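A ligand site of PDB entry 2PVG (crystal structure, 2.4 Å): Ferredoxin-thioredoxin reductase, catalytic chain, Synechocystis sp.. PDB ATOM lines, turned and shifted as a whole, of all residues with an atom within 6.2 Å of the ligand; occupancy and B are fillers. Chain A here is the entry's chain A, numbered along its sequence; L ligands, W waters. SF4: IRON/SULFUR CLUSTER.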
ATOM      1  N   PHE A  10       5.844 -32.036  -1.334  1.00  0.00           N
ATOM      2  CA  PHE A  10       6.179 -30.852  -2.105  1.00  0.00           C
ATOM      3  C   PHE A  10       7.416 -31.150  -2.943  1.00  0.00           C
ATOM      4  O   PHE A  10       7.379 -31.080  -4.170  1.00  0.00           O
ATOM      5  CB  PHE A  10       6.467 -29.668  -1.186  1.00  0.00           C
ATOM      6  CG  PHE A  10       7.246 -28.578  -1.838  1.00  0.00           C
ATOM      7  CD1 PHE A  10       6.692 -27.825  -2.857  1.00  0.00           C
ATOM      8  CD2 PHE A  10       8.555 -28.315  -1.444  1.00  0.00           C
ATOM      9  CE1 PHE A  10       7.434 -26.822  -3.487  1.00  0.00           C
ATOM     10  CE2 PHE A  10       9.305 -27.322  -2.068  1.00  0.00           C
ATOM     11  CZ  PHE A  10       8.741 -26.567  -3.088  1.00  0.00           C
ATOM     12  N   TYR A  14       7.600 -30.868  -6.894  1.00  0.00           N
ATOM     13  CA  TYR A  14       8.385 -29.766  -7.435  1.00  0.00           C
ATOM     14  C   TYR A  14       9.497 -30.269  -8.347  1.00  0.00           C
ATOM     15  O   TYR A  14       9.737 -29.699  -9.428  1.00  0.00           O
ATOM     16  CB  TYR A  14       8.997 -28.962  -6.299  1.00  0.00           C
ATOM     17  CG  TYR A  14       9.728 -27.747  -6.779  1.00  0.00           C
ATOM     18  CD1 TYR A  14      11.113 -27.719  -6.859  1.00  0.00           C
ATOM     19  CD2 TYR A  14       9.015 -26.613  -7.189  1.00  0.00           C
ATOM     20  CE1 TYR A  14      11.777 -26.596  -7.335  1.00  0.00           C
ATOM     21  CE2 TYR A  14       9.668 -25.493  -7.674  1.00  0.00           C
ATOM     22  CZ  TYR A  14      11.040 -25.474  -7.735  1.00  0.00           C
ATOM     23  OH  TYR A  14      11.653 -24.345  -8.199  1.00  0.00           O
ATOM     24  N   VAL A  32      17.543 -32.523   3.977  1.00  0.00           N
ATOM     25  CA  VAL A  32      17.022 -31.208   3.628  1.00  0.00           C
ATOM     26  C   VAL A  32      15.530 -31.139   3.927  1.00  0.00           C
ATOM     27  O   VAL A  32      15.057 -30.192   4.546  1.00  0.00           O
ATOM     28  CB  VAL A  32      17.257 -30.855   2.128  1.00  0.00           C
ATOM     29  CG1 VAL A  32      16.606 -29.527   1.791  1.00  0.00           C
ATOM     30  CG2 VAL A  32      18.728 -30.813   1.842  1.00  0.00           C
ATOM     31  N   LEU A  36      13.549 -28.502   6.226  1.00  0.00           N
ATOM     32  CA  LEU A  36      12.467 -27.690   5.703  1.00  0.00           C
ATOM     33  C   LEU A  36      11.220 -27.822   6.572  1.00  0.00           C
ATOM     34  O   LEU A  36      10.587 -26.826   6.953  1.00  0.00           O
ATOM     35  CB  LEU A  36      12.148 -28.113   4.265  1.00  0.00           C
ATOM     36  CG  LEU A  36      13.257 -27.836   3.238  1.00  0.00           C
ATOM     37  CD1 LEU A  36      13.052 -28.680   1.996  1.00  0.00           C
ATOM     38  CD2 LEU A  36      13.256 -26.355   2.893  1.00  0.00           C
ATOM     39  N   PRO A  46       8.658 -22.988   5.057  1.00  0.00           N
ATOM     40  CA  PRO A  46       9.820 -23.861   4.909  1.00  0.00           C
ATOM     41  C   PRO A  46      11.093 -23.099   4.536  1.00  0.00           C
ATOM     42  O   PRO A  46      11.563 -23.174   3.408  1.00  0.00           O
ATOM     43  CB  PRO A  46       9.387 -24.839   3.828  1.00  0.00           C
ATOM     44  CG  PRO A  46       8.469 -24.010   2.985  1.00  0.00           C
ATOM     45  CD  PRO A  46       7.658 -23.276   4.015  1.00  0.00           C
ATOM     46  N   LEU A  47      11.640 -22.366   5.507  1.00  0.00           N
ATOM     47  CA  LEU A  47      12.846 -21.588   5.282  1.00  0.00           C
ATOM     48  C   LEU A  47      14.039 -22.496   5.000  1.00  0.00           C
ATOM     49  O   LEU A  47      14.199 -23.524   5.638  1.00  0.00           O
ATOM     50  CB  LEU A  47      13.135 -20.734   6.513  1.00  0.00           C
ATOM     51  CG  LEU A  47      14.366 -19.848   6.385  1.00  0.00           C
ATOM     52  CD1 LEU A  47      14.186 -18.878   5.212  1.00  0.00           C
ATOM     53  CD2 LEU A  47      14.573 -19.085   7.691  1.00  0.00           C
ATOM     54  N   CYS A  48      14.880 -22.114   4.041  1.00  0.00           N
ATOM     55  CA  CYS A  48      16.021 -22.938   3.684  1.00  0.00           C
ATOM     56  C   CYS A  48      16.775 -23.369   4.923  1.00  0.00           C
ATOM     57  O   CYS A  48      17.205 -22.551   5.725  1.00  0.00           O
ATOM     58  CB  CYS A  48      16.950 -22.180   2.749  1.00  0.00           C
ATOM     59  SG  CYS A  48      18.125 -23.262   1.888  1.00  0.00           S
ATOM     60  N   PRO A  49      16.961 -24.682   5.087  1.00  0.00           N
ATOM     61  CA  PRO A  49      17.671 -25.209   6.260  1.00  0.00           C
ATOM     62  C   PRO A  49      19.193 -25.198   6.219  1.00  0.00           C
ATOM     63  O   PRO A  49      19.837 -24.969   7.238  1.00  0.00           O
ATOM     64  CB  PRO A  49      17.106 -26.620   6.392  1.00  0.00           C
ATOM     65  CG  PRO A  49      16.944 -27.019   4.952  1.00  0.00           C
ATOM     66  CD  PRO A  49      16.356 -25.776   4.308  1.00  0.00           C
ATOM     67  N   CYS A  50      19.775 -25.452   5.045  1.00  0.00           N
ATOM     68  CA  CYS A  50      21.224 -25.483   4.916  1.00  0.00           C
ATOM     69  C   CYS A  50      21.914 -24.107   4.956  1.00  0.00           C
ATOM     70  O   CYS A  50      22.876 -23.874   4.218  1.00  0.00           O
ATOM     71  CB  CYS A  50      21.620 -26.228   3.620  1.00  0.00           C
ATOM     72  SG  CYS A  50      21.237 -25.391   2.033  1.00  0.00           S
ATOM     73  N   ARG A  51      21.438 -23.211   5.811  1.00  0.00           N
ATOM     74  CA  ARG A  51      22.035 -21.878   5.920  1.00  0.00           C
ATOM     75  C   ARG A  51      21.941 -21.328   7.337  1.00  0.00           C
ATOM     76  O   ARG A  51      21.196 -21.839   8.171  1.00  0.00           O
ATOM     77  CB  ARG A  51      21.337 -20.882   4.978  1.00  0.00           C
ATOM     78  CG  ARG A  51      21.227 -21.284   3.513  1.00  0.00           C
ATOM     79  CD  ARG A  51      20.530 -20.186   2.708  1.00  0.00           C
ATOM     80  NE  ARG A  51      21.404 -19.034   2.547  1.00  0.00           N
ATOM     81  CZ  ARG A  51      22.439 -18.996   1.705  1.00  0.00           C
ATOM     82  NH1 ARG A  51      22.727 -20.045   0.961  1.00  0.00           N
ATOM     83  NH2 ARG A  51      23.203 -17.912   1.644  1.00  0.00           N
ATOM     84  N   TRP A  65      14.544 -16.558   1.056  1.00  0.00           N
ATOM     85  CA  TRP A  65      15.012 -17.916   1.304  1.00  0.00           C
ATOM     86  C   TRP A  65      13.921 -18.915   1.640  1.00  0.00           C
ATOM     87  O   TRP A  65      14.195 -19.947   2.238  1.00  0.00           O
ATOM     88  CB  TRP A  65      16.086 -17.931   2.395  1.00  0.00           C
ATOM     89  CG  TRP A  65      17.380 -17.350   1.959  1.00  0.00           C
ATOM     90  CD1 TRP A  65      18.016 -16.277   2.499  1.00  0.00           C
ATOM     91  CD2 TRP A  65      18.220 -17.827   0.903  1.00  0.00           C
ATOM     92  NE1 TRP A  65      19.206 -16.049   1.846  1.00  0.00           N
ATOM     93  CE2 TRP A  65      19.356 -16.986   0.858  1.00  0.00           C
ATOM     94  CE3 TRP A  65      18.130 -18.884  -0.015  1.00  0.00           C
ATOM     95  CZ2 TRP A  65      20.395 -17.174  -0.064  1.00  0.00           C
ATOM     96  CZ3 TRP A  65      19.159 -19.064  -0.930  1.00  0.00           C
ATOM     97  CH2 TRP A  65      20.285 -18.214  -0.945  1.00  0.00           C
ATOM     98  N   ASN A  66      12.675 -18.613   1.270  1.00  0.00           N
ATOM     99  CA  ASN A  66      11.613 -19.583   1.550  1.00  0.00           C
ATOM    100  C   ASN A  66      11.609 -20.577   0.405  1.00  0.00           C
ATOM    101  O   ASN A  66      11.524 -20.191  -0.750  1.00  0.00           O
ATOM    102  CB  ASN A  66      10.233 -18.909   1.674  1.00  0.00           C
ATOM    103  CG  ASN A  66      10.118 -18.037   2.905  1.00  0.00           C
ATOM    104  OD1 ASN A  66      10.882 -18.174   3.856  1.00  0.00           O
ATOM    105  ND2 ASN A  66       9.144 -17.136   2.903  1.00  0.00           N
ATOM    106  N   CYS A  67      11.741 -21.851   0.739  1.00  0.00           N
ATOM    107  CA  CYS A  67      11.750 -22.892  -0.268  1.00  0.00           C
ATOM    108  C   CYS A  67      10.418 -22.946  -0.999  1.00  0.00           C
ATOM    109  O   CYS A  67       9.356 -22.980  -0.362  1.00  0.00           O
ATOM    110  CB  CYS A  67      12.033 -24.234   0.399  1.00  0.00           C
ATOM    111  SG  CYS A  67      12.400 -25.534  -0.748  1.00  0.00           S
ATOM    112  N   PRO A  68      10.446 -22.949  -2.351  1.00  0.00           N
ATOM    113  CA  PRO A  68      11.667 -22.884  -3.163  1.00  0.00           C
ATOM    114  C   PRO A  68      12.136 -21.432  -3.267  1.00  0.00           C
ATOM    115  O   PRO A  68      11.366 -20.542  -3.657  1.00  0.00           O
ATOM    116  CB  PRO A  68      11.199 -23.472  -4.495  1.00  0.00           C
ATOM    117  CG  PRO A  68       9.809 -22.978  -4.589  1.00  0.00           C
ATOM    118  CD  PRO A  68       9.275 -23.218  -3.203  1.00  0.00           C
ATOM    119  N   CYS A  69      13.396 -21.217  -2.887  1.00  0.00           N
ATOM    120  CA  CYS A  69      14.007 -19.889  -2.871  1.00  0.00           C
ATOM    121  C   CYS A  69      14.179 -19.235  -4.254  1.00  0.00           C
ATOM    122  O   CYS A  69      14.095 -19.908  -5.292  1.00  0.00           O
ATOM    123  CB  CYS A  69      15.388 -19.975  -2.207  1.00  0.00           C
ATOM    124  SG  CYS A  69      16.598 -20.915  -3.210  1.00  0.00           S
ATOM    125  N   VAL A  70      14.451 -17.926  -4.252  1.00  0.00           N
ATOM    126  CA  VAL A  70      14.672 -17.181  -5.482  1.00  0.00           C
ATOM    127  C   VAL A  70      15.753 -17.800  -6.413  1.00  0.00           C
ATOM    128  O   VAL A  70      15.521 -18.004  -7.604  1.00  0.00           O
ATOM    129  CB  VAL A  70      15.027 -15.715  -5.181  1.00  0.00           C
ATOM    130  CG1 VAL A  70      15.324 -14.967  -6.490  1.00  0.00           C
ATOM    131  CG2 VAL A  70      13.845 -15.048  -4.468  1.00  0.00           C
ATOM    132  N   PRO A  71      16.934 -18.127  -5.865  1.00  0.00           N
ATOM    133  CA  PRO A  71      17.976 -18.711  -6.720  1.00  0.00           C
ATOM    134  C   PRO A  71      17.490 -19.971  -7.434  1.00  0.00           C
ATOM    135  O   PRO A  71      17.882 -20.251  -8.567  1.00  0.00           O
ATOM    136  CB  PRO A  71      19.102 -19.027  -5.734  1.00  0.00           C
ATOM    137  CG  PRO A  71      18.948 -17.986  -4.683  1.00  0.00           C
ATOM    138  CD  PRO A  71      17.427 -17.941  -4.486  1.00  0.00           C
ATOM    139  N   MET A  72      16.636 -20.742  -6.770  1.00  0.00           N
ATOM    140  CA  MET A  72      16.127 -21.974  -7.357  1.00  0.00           C
ATOM    141  C   MET A  72      15.009 -21.737  -8.387  1.00  0.00           C
ATOM    142  O   MET A  72      14.955 -22.411  -9.415  1.00  0.00           O
ATOM    143  CB  MET A  72      15.625 -22.910  -6.272  1.00  0.00           C
ATOM    144  CG  MET A  72      15.028 -24.214  -6.795  1.00  0.00           C
ATOM    145  SD  MET A  72      16.251 -25.200  -7.662  1.00  0.00           S
ATOM    146  CE  MET A  72      15.227 -26.091  -8.811  1.00  0.00           C
ATOM    147  N   GLU A  77      19.135 -22.969  -8.975  1.00  0.00           N
ATOM    148  CA  GLU A  77      20.314 -23.163  -8.155  1.00  0.00           C
ATOM    149  C   GLU A  77      19.867 -23.476  -6.739  1.00  0.00           C
ATOM    150  O   GLU A  77      19.437 -22.586  -5.990  1.00  0.00           O
ATOM    151  CB  GLU A  77      21.194 -21.924  -8.146  1.00  0.00           C
ATOM    152  CG  GLU A  77      21.639 -21.501  -9.526  1.00  0.00           C
ATOM    153  CD  GLU A  77      22.840 -20.572  -9.525  1.00  0.00           C
ATOM    154  OE1 GLU A  77      22.850 -19.600  -8.725  1.00  0.00           O
ATOM    155  OE2 GLU A  77      23.761 -20.806 -10.338  1.00  0.00           O
ATOM    156  N   CYS A  78      19.944 -24.766  -6.392  1.00  0.00           N
ATOM    157  CA  CYS A  78      19.564 -25.250  -5.083  1.00  0.00           C
ATOM    158  C   CYS A  78      20.823 -25.513  -4.284  1.00  0.00           C
ATOM    159  O   CYS A  78      21.466 -26.549  -4.448  1.00  0.00           O
ATOM    160  CB  CYS A  78      18.751 -26.549  -5.214  1.00  0.00           C
ATOM    161  SG  CYS A  78      18.308 -27.341  -3.653  1.00  0.00           S
ATOM    162  N   HIS A  79      21.179 -24.578  -3.422  1.00  0.00           N
ATOM    163  CA  HIS A  79      22.383 -24.752  -2.618  1.00  0.00           C
ATOM    164  C   HIS A  79      22.366 -25.990  -1.712  1.00  0.00           C
ATOM    165  O   HIS A  79      23.402 -26.592  -1.478  1.00  0.00           O
ATOM    166  CB  HIS A  79      22.644 -23.516  -1.778  1.00  0.00           C
ATOM    167  CG  HIS A  79      23.882 -23.606  -0.947  1.00  0.00           C
ATOM    168  ND1 HIS A  79      25.098 -24.023  -1.455  1.00  0.00           N
ATOM    169  CD2 HIS A  79      24.110 -23.284   0.347  1.00  0.00           C
ATOM    170  CE1 HIS A  79      26.014 -23.947  -0.521  1.00  0.00           C
ATOM    171  NE2 HIS A  79      25.450 -23.508   0.590  1.00  0.00           N
ATOM    172  N   CYS A  80      21.186 -26.370  -1.212  1.00  0.00           N
ATOM    173  CA  CYS A  80      21.102 -27.534  -0.327  1.00  0.00           C
ATOM    174  C   CYS A  80      21.289 -28.853  -1.068  1.00  0.00           C
ATOM    175  O   CYS A  80      21.280 -29.915  -0.445  1.00  0.00           O
ATOM    176  CB  CYS A  80      19.768 -27.572   0.415  1.00  0.00           C
ATOM    177  SG  CYS A  80      19.419 -26.148   1.479  1.00  0.00           S
ATOM    178  N   MET A  81      21.443 -28.769  -2.376  1.00  0.00           N
ATOM    179  CA  MET A  81      21.616 -29.966  -3.195  1.00  0.00           C
ATOM    180  C   MET A  81      20.329 -30.774  -3.245  1.00  0.00           C
ATOM    181  O   MET A  81      20.337 -31.919  -3.694  1.00  0.00           O
ATOM    182  CB  MET A  81      22.748 -30.834  -2.650  1.00  0.00           C
ATOM    183  CG  MET A  81      24.124 -30.204  -2.764  1.00  0.00           C
ATOM    184  SD  MET A  81      24.581 -29.989  -4.488  1.00  0.00           S
ATOM    185  CE  MET A  81      24.226 -28.245  -4.743  1.00  0.00           C
ATOM    186  N   LEU A  82      19.228 -30.187  -2.772  1.00  0.00           N
ATOM    187  CA  LEU A  82      17.946 -30.901  -2.788  1.00  0.00           C
ATOM    188  C   LEU A  82      17.446 -31.136  -4.207  1.00  0.00           C
ATOM    189  O   LEU A  82      17.097 -32.258  -4.576  1.00  0.00           O
ATOM    190  CB  LEU A  82      16.892 -30.114  -1.981  1.00  0.00           C
ATOM    191  CG  LEU A  82      15.436 -30.578  -2.066  1.00  0.00           C
ATOM    192  CD1 LEU A  82      15.326 -32.048  -1.686  1.00  0.00           C
ATOM    193  CD2 LEU A  82      14.581 -29.734  -1.142  1.00  0.00           C
ATOM    194  N   PHE A  83      17.415 -30.067  -4.998  1.00  0.00           N
ATOM    195  CA  PHE A  83      16.951 -30.106  -6.403  1.00  0.00           C
ATOM    196  C   PHE A  83      18.113 -29.915  -7.377  1.00  0.00           C
ATOM    197  O   PHE A  83      18.757 -28.858  -7.390  1.00  0.00           O
ATOM    198  CB  PHE A  83      15.906 -28.997  -6.632  1.00  0.00           C
ATOM    199  CG  PHE A  83      14.701 -29.117  -5.750  1.00  0.00           C
ATOM    200  CD1 PHE A  83      14.311 -28.049  -4.940  1.00  0.00           C
ATOM    201  CD2 PHE A  83      13.962 -30.295  -5.712  1.00  0.00           C
ATOM    202  CE1 PHE A  83      13.209 -28.173  -4.085  1.00  0.00           C
ATOM    203  CE2 PHE A  83      12.869 -30.427  -4.865  1.00  0.00           C
ATOM    204  CZ  PHE A  83      12.488 -29.366  -4.063  1.00  0.00           C
HETATM  205 FE1  SF4 L   1      17.234 -25.656  -2.258  1.00  0.00          FE
HETATM  206 FE2  SF4 L   1      14.759 -25.087  -1.173  1.00  0.00          FE
HETATM  207 FE3  SF4 L   1      16.407 -23.083  -2.106  1.00  0.00          FE
HETATM  208 FE4  SF4 L   1      17.099 -24.452   0.181  1.00  0.00          FE
HETATM  209  S1  SF4 L   1      15.221 -23.085  -0.142  1.00  0.00           S
HETATM  210  S2  SF4 L   1      18.501 -23.869  -1.554  1.00  0.00           S
HETATM  211  S3  SF4 L   1      16.332 -26.559  -0.322  1.00  0.00           S
HETATM  212  S4  SF4 L   1      15.439 -24.756  -3.381  1.00  0.00           S
HETATM  213  O   HOH W   1      20.595 -21.988   0.448  1.00  0.00           O
HETATM  214  O   HOH W   2      20.125 -21.838  -3.041  1.00  0.00           O
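An iron atom (FE4) of the ligand is bound by the side-chain sulfur (SG) of Cys 48, 2.3 Å away.
The side-chain sulfur (SG) of Cys 78 binds an iron atom (FE1) of the ligand (2.4 Å).
N of Cys 67 lies close to S1 of the ligand (3.8 Å).
SG of Cys 67 is bound to FE2 of the ligand (2.4 Å).
The backbone NH (N) of Cys 69 sits close to a sulfur (S1) of the ligand (3.8 Å).
SG of Cys 69 is bound to FE3 of the ligand (2.4 Å).
A sulfur (S2) of the ligand sits close to the backbone NH (N) of Cys 80 (3.7 Å).
The backbone NH (N) of His 79 sits close to a sulfur (S2) of the ligand (3.3 Å).
SG of Cys 80 lies close to SG of Cys 48 (3.2 Å).
The backbone NH of Cys 48 is in hydrogen-bond range of the backbone carbonyl oxygen of Trp 65, 2.9 Å away.
SG of Cys 50 lies close to SG of Cys 48, at 3.8 Å.
SG of Cys 78 lies close to N of Leu 82, 3.1 Å away.
The side-chain sulfur of Cys 78 sits close to the backbone NH of Phe 83.
N of Met 81 sits close to SG of Cys 78.
SG of Cys 69 sits close to N of Met 72, 3.6 Å away.
The side-chain sulfur (SG) of Cys 50 is disulfide-bonded to the side-chain sulfur (SG) of Cys 80 (2.0 Å).
Merely in contact with the ligand: Val 32 (3.7 Å), Met 72 (3.4 Å), Leu 82 (3.7 Å) and Phe 83 (3.8 Å).
Ten residues have an atom within 4 Å of the ligand: Val 32, Cys 48, Cys 67, Cys 69, Met 72, Cys 78, His 79, Cys 80, Leu 82 and Phe 83.
Water W2 lies within hydrogen-bond range of the backbone NH of His 79, a sulfur (S2) of the ligand and the backbone carbonyl oxygen of Glu 77.
Water W1 bridges NH1 of Arg 51 (2.9 Å) and S2 of the ligand (3.5 Å).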
